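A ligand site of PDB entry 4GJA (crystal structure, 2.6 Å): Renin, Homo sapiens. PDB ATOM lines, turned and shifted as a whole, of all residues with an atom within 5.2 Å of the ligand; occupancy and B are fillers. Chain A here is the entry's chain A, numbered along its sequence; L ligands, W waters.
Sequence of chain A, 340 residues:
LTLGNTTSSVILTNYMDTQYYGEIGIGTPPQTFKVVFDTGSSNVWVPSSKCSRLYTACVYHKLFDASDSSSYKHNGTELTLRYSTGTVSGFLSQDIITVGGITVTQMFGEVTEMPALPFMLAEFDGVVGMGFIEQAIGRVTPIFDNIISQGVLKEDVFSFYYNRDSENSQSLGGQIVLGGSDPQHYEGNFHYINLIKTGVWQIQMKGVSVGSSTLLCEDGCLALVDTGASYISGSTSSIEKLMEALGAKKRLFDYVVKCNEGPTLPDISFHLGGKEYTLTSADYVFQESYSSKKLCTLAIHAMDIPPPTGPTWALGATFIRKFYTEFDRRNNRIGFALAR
The backbone NH (N) of Ser 84 sits at hydrogen-bond distance from an oxygen (O3) of the ligand (3.2 Å). The side-chain hydroxyl of Ser 84 sits at hydrogen-bond distance from an oxygen (O3) of the ligand, at 2.7 Å. O of Gly 228 lies within hydrogen-bond range of N3 of the ligand (3.2 Å). A nitrogen (N2) of the ligand lies within salt-bridge range of the side-chain carboxylate (OD2) of Asp 226 (2.8 Å). The side-chain carboxylate (OD1) of Asp 38 is in salt-bridge range of a nitrogen (N2) of the ligand (2.8 Å).
OD1 of Asp 226 lies within hydrogen-bond range of N of Gly 228 (3.0 Å). The side-chain carboxylate of Asp 38 sits close to the backbone NH of Gly 228, 3.4 Å away. The side-chain hydroxyl (OG) of Ser 41 is in hydrogen-bond range of the side-chain carboxylate (OD2) of Asp 38, at 2.6 Å. N of Gly 40 sits at hydrogen-bond distance from OD1 of Asp 226 (3.2 Å). The side-chain carboxylate of Asp 38 sits at hydrogen-bond distance from the backbone NH of Gly 40 (2.9 Å). OD1 of Asp 226 lies close to OD1 of Asp 38 (2.6 Å). The backbone carbonyl oxygen (O) of Leu 121 sits at hydrogen-bond distance from the side-chain amide nitrogen (NE2) of Gln 19, 3.0 Å away.
Water W2 bridges O2 of the ligand (2.7 Å) and O of Gly 40 (2.9 Å). Water W1 bridges the backbone carbonyl oxygen (O) of Arg 82 (3.0 Å) and a nitrogen (N1) of the ligand (3.0 Å). Water W3 bridges OD2 of Asp 226 (2.9 Å) and O1 of the ligand (3.1 Å). Water W4 lies within hydrogen-bond range of N of Ser 230 (3.2 Å) and N3 of the ligand (3.4 Å).
Merely in contact with the ligand: Val 127, Tyr 83, Gln 19, Pro 306, Gly 40, Ile 305, Met 303, Thr 85, Pro 118, Phe 124, Val 36, Ala 122 and Leu 224. Within 4 Å of the ligand: Gln 19, Val 36, Asp 38, Gly 40, Tyr 83, Ser 84, Thr 85, Pro 118, Ala 122, Phe 124, Val 127, Leu 224, Asp 226, Gly 228, Met 303, Ile 305 and Pro 306. The nearest printed residue that does not touch the ligand is Arg 82 (4.01 Å).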
ATOM      1  N   GLN A  19     -23.643  10.229 -22.177  1.00  0.00           N
ATOM      2  CA  GLN A  19     -23.448  10.449 -20.743  1.00  0.00           C
ATOM      3  C   GLN A  19     -24.788  10.446 -20.058  1.00  0.00           C
ATOM      4  O   GLN A  19     -25.688  11.146 -20.497  1.00  0.00           O
ATOM      5  CB  GLN A  19     -22.718  11.763 -20.489  1.00  0.00           C
ATOM      6  CG  GLN A  19     -21.291  11.778 -21.035  1.00  0.00           C
ATOM      7  CD  GLN A  19     -20.690  13.139 -20.958  1.00  0.00           C
ATOM      8  OE1 GLN A  19     -20.871  13.840 -19.964  1.00  0.00           O
ATOM      9  NE2 GLN A  19     -19.971  13.534 -22.004  1.00  0.00           N
ATOM     10  N   VAL A  36     -21.979  10.035 -12.682  1.00  0.00           N
ATOM     11  CA  VAL A  36     -22.177   8.868 -13.514  1.00  0.00           C
ATOM     12  C   VAL A  36     -22.111   7.656 -12.568  1.00  0.00           C
ATOM     13  O   VAL A  36     -21.175   7.561 -11.770  1.00  0.00           O
ATOM     14  CB  VAL A  36     -21.087   8.835 -14.603  1.00  0.00           C
ATOM     15  CG1 VAL A  36     -20.825   7.426 -15.099  1.00  0.00           C
ATOM     16  CG2 VAL A  36     -21.460   9.729 -15.758  1.00  0.00           C
ATOM     17  N   ASP A  38     -21.287   4.120 -12.361  1.00  0.00           N
ATOM     18  CA  ASP A  38     -20.413   3.232 -13.120  1.00  0.00           C
ATOM     19  C   ASP A  38     -20.209   1.825 -12.513  1.00  0.00           C
ATOM     20  O   ASP A  38     -19.605   1.707 -11.451  1.00  0.00           O
ATOM     21  CB  ASP A  38     -19.058   3.970 -13.347  1.00  0.00           C
ATOM     22  CG  ASP A  38     -17.987   3.200 -14.074  1.00  0.00           C
ATOM     23  OD1 ASP A  38     -18.326   2.303 -14.845  1.00  0.00           O
ATOM     24  OD2 ASP A  38     -16.806   3.564 -13.923  1.00  0.00           O
ATOM     25  N   GLY A  40     -18.389  -0.488 -13.948  1.00  0.00           N
ATOM     26  CA  GLY A  40     -17.024  -0.827 -14.306  1.00  0.00           C
ATOM     27  C   GLY A  40     -15.967  -0.373 -13.321  1.00  0.00           C
ATOM     28  O   GLY A  40     -14.782  -0.672 -13.523  1.00  0.00           O
ATOM     29  N   SER A  41     -16.342   0.359 -12.250  1.00  0.00           N
ATOM     30  CA  SER A  41     -15.414   0.862 -11.221  1.00  0.00           C
ATOM     31  C   SER A  41     -16.076   0.844  -9.833  1.00  0.00           C
ATOM     32  O   SER A  41     -17.293   0.635  -9.756  1.00  0.00           O
ATOM     33  CB  SER A  41     -14.871   2.242 -11.574  1.00  0.00           C
ATOM     34  OG  SER A  41     -15.892   3.237 -11.563  1.00  0.00           O
ATOM     35  N   ARG A  82      -7.522   5.081 -12.562  1.00  0.00           N
ATOM     36  CA  ARG A  82      -7.297   4.976 -13.997  1.00  0.00           C
ATOM     37  C   ARG A  82      -8.536   4.532 -14.717  1.00  0.00           C
ATOM     38  O   ARG A  82      -9.229   3.617 -14.260  1.00  0.00           O
ATOM     39  CB  ARG A  82      -6.038   4.141 -14.316  1.00  0.00           C
ATOM     40  CG  ARG A  82      -4.764   4.960 -14.080  1.00  0.00           C
ATOM     41  CD  ARG A  82      -3.459   4.160 -14.148  1.00  0.00           C
ATOM     42  NE  ARG A  82      -2.406   4.844 -13.374  1.00  0.00           N
ATOM     43  CZ  ARG A  82      -2.084   4.563 -12.111  1.00  0.00           C
ATOM     44  NH1 ARG A  82      -1.153   5.273 -11.475  1.00  0.00           N
ATOM     45  NH2 ARG A  82      -2.711   3.585 -11.453  1.00  0.00           N
ATOM     46  N   TYR A  83      -8.859   5.233 -15.799  1.00  0.00           N
ATOM     47  CA  TYR A  83     -10.033   4.921 -16.610  1.00  0.00           C
ATOM     48  C   TYR A  83      -9.576   4.774 -18.064  1.00  0.00           C
ATOM     49  O   TYR A  83      -8.389   4.905 -18.376  1.00  0.00           O
ATOM     50  CB  TYR A  83     -11.140   6.000 -16.431  1.00  0.00           C
ATOM     51  CG  TYR A  83     -11.677   6.103 -15.017  1.00  0.00           C
ATOM     52  CD1 TYR A  83     -12.560   5.152 -14.518  1.00  0.00           C
ATOM     53  CD2 TYR A  83     -11.302   7.155 -14.180  1.00  0.00           C
ATOM     54  CE1 TYR A  83     -13.057   5.232 -13.215  1.00  0.00           C
ATOM     55  CE2 TYR A  83     -11.766   7.230 -12.861  1.00  0.00           C
ATOM     56  CZ  TYR A  83     -12.662   6.276 -12.397  1.00  0.00           C
ATOM     57  OH  TYR A  83     -13.163   6.348 -11.129  1.00  0.00           O
ATOM     58  N   SER A  84     -10.501   4.506 -18.943  1.00  0.00           N
ATOM     59  CA  SER A  84     -10.141   4.302 -20.306  1.00  0.00           C
ATOM     60  C   SER A  84      -9.655   5.557 -21.018  1.00  0.00           C
ATOM     61  O   SER A  84      -8.628   5.523 -21.701  1.00  0.00           O
ATOM     62  CB  SER A  84     -11.304   3.641 -21.037  1.00  0.00           C
ATOM     63  OG  SER A  84     -12.399   4.515 -21.271  1.00  0.00           O
ATOM     64  N   THR A  85     -10.380   6.648 -20.841  1.00  0.00           N
ATOM     65  CA  THR A  85     -10.201   7.945 -21.499  1.00  0.00           C
ATOM     66  C   THR A  85      -9.099   8.815 -20.923  1.00  0.00           C
ATOM     67  O   THR A  85      -8.614   9.733 -21.597  1.00  0.00           O
ATOM     68  CB  THR A  85     -11.530   8.715 -21.411  1.00  0.00           C
ATOM     69  OG1 THR A  85     -11.982   8.660 -20.045  1.00  0.00           O
ATOM     70  CG2 THR A  85     -12.585   8.165 -22.355  1.00  0.00           C
ATOM     71  N   PRO A 118     -10.217  13.842 -20.717  1.00  0.00           N
ATOM     72  CA  PRO A 118     -11.565  14.042 -21.271  1.00  0.00           C
ATOM     73  C   PRO A 118     -12.531  14.897 -20.426  1.00  0.00           C
ATOM     74  O   PRO A 118     -13.671  15.087 -20.839  1.00  0.00           O
ATOM     75  CB  PRO A 118     -12.073  12.589 -21.348  1.00  0.00           C
ATOM     76  CG  PRO A 118     -11.552  12.007 -20.044  1.00  0.00           C
ATOM     77  CD  PRO A 118     -10.185  12.646 -19.849  1.00  0.00           C
ATOM     78  N   PHE A 119     -12.110  15.352 -19.243  1.00  0.00           N
ATOM     79  CA  PHE A 119     -13.027  16.010 -18.316  1.00  0.00           C
ATOM     80  C   PHE A 119     -13.702  17.319 -18.740  1.00  0.00           C
ATOM     81  O   PHE A 119     -14.762  17.615 -18.204  1.00  0.00           O
ATOM     82  CB  PHE A 119     -12.537  15.941 -16.848  1.00  0.00           C
ATOM     83  CG  PHE A 119     -12.308  14.482 -16.448  1.00  0.00           C
ATOM     84  CD1 PHE A 119     -13.396  13.636 -16.204  1.00  0.00           C
ATOM     85  CD2 PHE A 119     -11.026  13.924 -16.466  1.00  0.00           C
ATOM     86  CE1 PHE A 119     -13.185  12.276 -15.922  1.00  0.00           C
ATOM     87  CE2 PHE A 119     -10.833  12.553 -16.222  1.00  0.00           C
ATOM     88  CZ  PHE A 119     -11.908  11.746 -15.934  1.00  0.00           C
ATOM     89  N   LEU A 121     -15.103  17.533 -21.599  1.00  0.00           N
ATOM     90  CA  LEU A 121     -16.194  16.964 -22.398  1.00  0.00           C
ATOM     91  C   LEU A 121     -17.282  16.360 -21.497  1.00  0.00           C
ATOM     92  O   LEU A 121     -18.355  16.012 -21.977  1.00  0.00           O
ATOM     93  CB  LEU A 121     -15.680  15.860 -23.333  1.00  0.00           C
ATOM     94  CG  LEU A 121     -14.495  16.136 -24.265  1.00  0.00           C
ATOM     95  CD1 LEU A 121     -14.074  14.844 -24.949  1.00  0.00           C
ATOM     96  CD2 LEU A 121     -14.810  17.220 -25.320  1.00  0.00           C
ATOM     97  N   ALA A 122     -16.990  16.243 -20.203  1.00  0.00           N
ATOM     98  CA  ALA A 122     -17.941  15.641 -19.292  1.00  0.00           C
ATOM     99  C   ALA A 122     -18.949  16.661 -18.818  1.00  0.00           C
ATOM    100  O   ALA A 122     -18.575  17.761 -18.392  1.00  0.00           O
ATOM    101  CB  ALA A 122     -17.220  15.017 -18.109  1.00  0.00           C
ATOM    102  N   PHE A 124     -21.076  15.675 -16.397  1.00  0.00           N
ATOM    103  CA  PHE A 124     -21.079  15.270 -14.986  1.00  0.00           C
ATOM    104  C   PHE A 124     -19.803  15.792 -14.303  1.00  0.00           C
ATOM    105  O   PHE A 124     -18.827  16.079 -14.986  1.00  0.00           O
ATOM    106  CB  PHE A 124     -21.175  13.733 -14.880  1.00  0.00           C
ATOM    107  CG  PHE A 124     -20.057  12.976 -15.593  1.00  0.00           C
ATOM    108  CD1 PHE A 124     -20.152  12.680 -16.947  1.00  0.00           C
ATOM    109  CD2 PHE A 124     -18.902  12.577 -14.909  1.00  0.00           C
ATOM    110  CE1 PHE A 124     -19.115  11.971 -17.605  1.00  0.00           C
ATOM    111  CE2 PHE A 124     -17.868  11.898 -15.571  1.00  0.00           C
ATOM    112  CZ  PHE A 124     -17.981  11.579 -16.903  1.00  0.00           C
ATOM    113  N   VAL A 127     -17.979  10.625 -10.237  1.00  0.00           N
ATOM    114  CA  VAL A 127     -18.325   9.223 -10.475  1.00  0.00           C
ATOM    115  C   VAL A 127     -18.742   8.517  -9.188  1.00  0.00           C
ATOM    116  O   VAL A 127     -18.194   8.794  -8.143  1.00  0.00           O
ATOM    117  CB  VAL A 127     -17.088   8.532 -11.145  1.00  0.00           C
ATOM    118  CG1 VAL A 127     -17.293   7.026 -11.310  1.00  0.00           C
ATOM    119  CG2 VAL A 127     -16.743   9.188 -12.470  1.00  0.00           C
ATOM    120  N   LEU A 224     -17.759  -7.352 -20.137  1.00  0.00           N
ATOM    121  CA  LEU A 224     -17.880  -6.470 -18.961  1.00  0.00           C
ATOM    122  C   LEU A 224     -19.181  -5.636 -19.147  1.00  0.00           C
ATOM    123  O   LEU A 224     -19.349  -4.975 -20.181  1.00  0.00           O
ATOM    124  CB  LEU A 224     -16.620  -5.563 -18.856  1.00  0.00           C
ATOM    125  CG  LEU A 224     -16.611  -4.541 -17.712  1.00  0.00           C
ATOM    126  CD1 LEU A 224     -16.491  -5.203 -16.331  1.00  0.00           C
ATOM    127  CD2 LEU A 224     -15.556  -3.486 -17.936  1.00  0.00           C
ATOM    128  N   ASP A 226     -20.744  -2.615 -18.426  1.00  0.00           N
ATOM    129  CA  ASP A 226     -20.288  -1.301 -17.972  1.00  0.00           C
ATOM    130  C   ASP A 226     -21.245  -0.109 -18.247  1.00  0.00           C
ATOM    131  O   ASP A 226     -21.258   0.453 -19.342  1.00  0.00           O
ATOM    132  CB  ASP A 226     -18.862  -1.034 -18.502  1.00  0.00           C
ATOM    133  CG  ASP A 226     -18.120   0.126 -17.881  1.00  0.00           C
ATOM    134  OD1 ASP A 226     -18.642   0.702 -16.901  1.00  0.00           O
ATOM    135  OD2 ASP A 226     -17.019   0.464 -18.365  1.00  0.00           O
ATOM    136  N   GLY A 228     -20.838   2.750 -17.111  1.00  0.00           N
ATOM    137  CA  GLY A 228     -19.917   3.886 -17.232  1.00  0.00           C
ATOM    138  C   GLY A 228     -19.327   4.078 -18.608  1.00  0.00           C
ATOM    139  O   GLY A 228     -18.692   5.084 -18.868  1.00  0.00           O
ATOM    140  N   ALA A 229     -19.514   3.107 -19.497  1.00  0.00           N
ATOM    141  CA  ALA A 229     -19.020   3.134 -20.870  1.00  0.00           C
ATOM    142  C   ALA A 229     -20.164   3.598 -21.769  1.00  0.00           C
ATOM    143  O   ALA A 229     -21.322   3.174 -21.581  1.00  0.00           O
ATOM    144  CB  ALA A 229     -18.519   1.754 -21.283  1.00  0.00           C
ATOM    145  N   SER A 230     -19.886   4.520 -22.669  1.00  0.00           N
ATOM    146  CA  SER A 230     -20.864   5.089 -23.578  1.00  0.00           C
ATOM    147  C   SER A 230     -21.227   4.148 -24.681  1.00  0.00           C
ATOM    148  O   SER A 230     -22.342   4.196 -25.174  1.00  0.00           O
ATOM    149  CB  SER A 230     -20.308   6.343 -24.221  1.00  0.00           C
ATOM    150  OG  SER A 230     -20.012   7.333 -23.248  1.00  0.00           O
ATOM    151  N   MET A 303     -11.336  -0.755 -27.895  1.00  0.00           N
ATOM    152  CA  MET A 303     -10.925  -0.452 -26.539  1.00  0.00           C
ATOM    153  C   MET A 303     -10.162  -1.648 -26.005  1.00  0.00           C
ATOM    154  O   MET A 303     -10.724  -2.733 -25.841  1.00  0.00           O
ATOM    155  CB  MET A 303     -12.171  -0.145 -25.697  1.00  0.00           C
ATOM    156  CG  MET A 303     -11.944   0.019 -24.248  1.00  0.00           C
ATOM    157  SD  MET A 303     -11.571   1.706 -23.833  1.00  0.00           S
ATOM    158  CE  MET A 303      -9.806   1.502 -23.434  1.00  0.00           C
ATOM    159  N   ASP A 304      -8.862  -1.470 -25.796  1.00  0.00           N
ATOM    160  CA  ASP A 304      -8.023  -2.548 -25.269  1.00  0.00           C
ATOM    161  C   ASP A 304      -7.938  -2.370 -23.765  1.00  0.00           C
ATOM    162  O   ASP A 304      -7.213  -1.513 -23.260  1.00  0.00           O
ATOM    163  CB  ASP A 304      -6.655  -2.626 -25.966  1.00  0.00           C
ATOM    164  CG  ASP A 304      -6.762  -2.785 -27.481  1.00  0.00           C
ATOM    165  OD1 ASP A 304      -6.537  -1.782 -28.197  1.00  0.00           O
ATOM    166  OD2 ASP A 304      -7.111  -3.903 -27.938  1.00  0.00           O
ATOM    167  N   ILE A 305      -8.828  -3.094 -23.078  1.00  0.00           N
ATOM    168  CA  ILE A 305      -8.959  -3.062 -21.628  1.00  0.00           C
ATOM    169  C   ILE A 305      -7.828  -3.912 -21.096  1.00  0.00           C
ATOM    170  O   ILE A 305      -7.636  -5.026 -21.593  1.00  0.00           O
ATOM    171  CB  ILE A 305     -10.381  -3.498 -21.167  1.00  0.00           C
ATOM    172  CG1 ILE A 305     -11.433  -2.469 -21.640  1.00  0.00           C
ATOM    173  CG2 ILE A 305     -10.442  -3.702 -19.639  1.00  0.00           C
ATOM    174  CD1 ILE A 305     -12.869  -2.938 -21.717  1.00  0.00           C
ATOM    175  N   PRO A 306      -6.994  -3.376 -20.176  1.00  0.00           N
ATOM    176  CA  PRO A 306      -5.836  -4.145 -19.703  1.00  0.00           C
ATOM    177  C   PRO A 306      -6.179  -5.267 -18.737  1.00  0.00           C
ATOM    178  O   PRO A 306      -7.257  -5.243 -18.132  1.00  0.00           O
ATOM    179  CB  PRO A 306      -4.969  -3.065 -19.039  1.00  0.00           C
ATOM    180  CG  PRO A 306      -5.938  -2.073 -18.531  1.00  0.00           C
ATOM    181  CD  PRO A 306      -7.048  -2.045 -19.533  1.00  0.00           C
ATOM    182  N   THR A 309      -8.806  -7.592 -15.786  1.00  0.00           N
ATOM    183  CA  THR A 309     -10.146  -7.402 -16.361  1.00  0.00           C
ATOM    184  C   THR A 309     -10.168  -7.745 -17.857  1.00  0.00           C
ATOM    185  O   THR A 309     -10.983  -8.567 -18.291  1.00  0.00           O
ATOM    186  CB  THR A 309     -10.684  -5.991 -15.993  1.00  0.00           C
ATOM    187  OG1 THR A 309     -10.728  -5.894 -14.570  1.00  0.00           O
ATOM    188  CG2 THR A 309     -12.073  -5.697 -16.577  1.00  0.00           C
HETATM  189  C1  LIG L   1      -6.871   2.078 -19.664  1.00  0.00           C
HETATM  190  C2  LIG L   1      -8.155   1.482 -19.113  1.00  0.00           C
HETATM  191  C3  LIG L   1      -8.399   1.490 -17.726  1.00  0.00           C
HETATM  192  C4  LIG L   1      -9.610   0.939 -17.222  1.00  0.00           C
HETATM  193  C5  LIG L   1     -10.562   0.414 -18.125  1.00  0.00           C
HETATM  194  C6  LIG L   1     -10.284   0.319 -19.482  1.00  0.00           C
HETATM  195  C7  LIG L   1      -9.083   0.842 -19.964  1.00  0.00           C
HETATM  196  S1  LIG L   1     -12.065  -0.365 -17.626  1.00  0.00           S
HETATM  197  O1  LIG L   1     -12.822  -0.753 -18.831  1.00  0.00           O
HETATM  198  O2  LIG L   1     -11.730  -1.394 -16.649  1.00  0.00           O
HETATM  199  N1  LIG L   1     -12.803   0.879 -16.838  1.00  0.00           N
HETATM  200  C8  LIG L   1     -14.017   1.520 -17.311  1.00  0.00           C
HETATM  201  C9  LIG L   1     -14.985   1.762 -16.124  1.00  0.00           C
HETATM  202  N2  LIG L   1     -16.167   2.493 -16.622  1.00  0.00           N
HETATM  203  C10 LIG L   1     -15.871   3.822 -17.214  1.00  0.00           C
HETATM  204  C11 LIG L   1     -14.916   3.660 -18.448  1.00  0.00           C
HETATM  205  C12 LIG L   1     -13.654   2.861 -18.021  1.00  0.00           C
HETATM  206  C13 LIG L   1     -14.625   5.031 -19.042  1.00  0.00           C
HETATM  207  O3  LIG L   1     -13.501   5.499 -18.954  1.00  0.00           O
HETATM  208  N3  LIG L   1     -15.658   5.687 -19.649  1.00  0.00           N
HETATM  209  C14 LIG L   1     -15.549   7.032 -20.238  1.00  0.00           C
HETATM  210  C15 LIG L   1     -16.314   8.045 -19.341  1.00  0.00           C
HETATM  211  C16 LIG L   1     -16.082   7.865 -17.844  1.00  0.00           C
HETATM  212  C17 LIG L   1     -17.161   7.383 -17.040  1.00  0.00           C
HETATM  213  C18 LIG L   1     -16.966   7.126 -15.674  1.00  0.00           C
HETATM  214  C19 LIG L   1     -15.687   7.303 -15.133  1.00  0.00           C
HETATM  215  C20 LIG L   1     -14.607   7.787 -15.915  1.00  0.00           C
HETATM  216  C21 LIG L   1     -14.803   8.045 -17.281  1.00  0.00           C
HETATM  217  C22 LIG L   1     -16.336   9.508 -19.829  1.00  0.00           C
HETATM  218  C23 LIG L   1     -17.346   9.951 -20.721  1.00  0.00           C
HETATM  219  C24 LIG L   1     -17.361  11.291 -21.173  1.00  0.00           C
HETATM  220  C25 LIG L   1     -16.372  12.196 -20.742  1.00  0.00           C
HETATM  221  C26 LIG L   1     -15.375  11.770 -19.838  1.00  0.00           C
HETATM  222  C27 LIG L   1     -15.355  10.419 -19.398  1.00  0.00           C
HETATM  223  O   HOH W   1     -11.616   1.819 -14.225  1.00  0.00           O
HETATM  224  O   HOH W   2     -13.439  -2.693 -15.034  1.00  0.00           O
HETATM  225  O   HOH W   3     -15.329  -0.294 -20.650  1.00  0.00           O
HETATM  226  O   HOH W   4     -16.777   5.308 -22.884  1.00  0.00           O
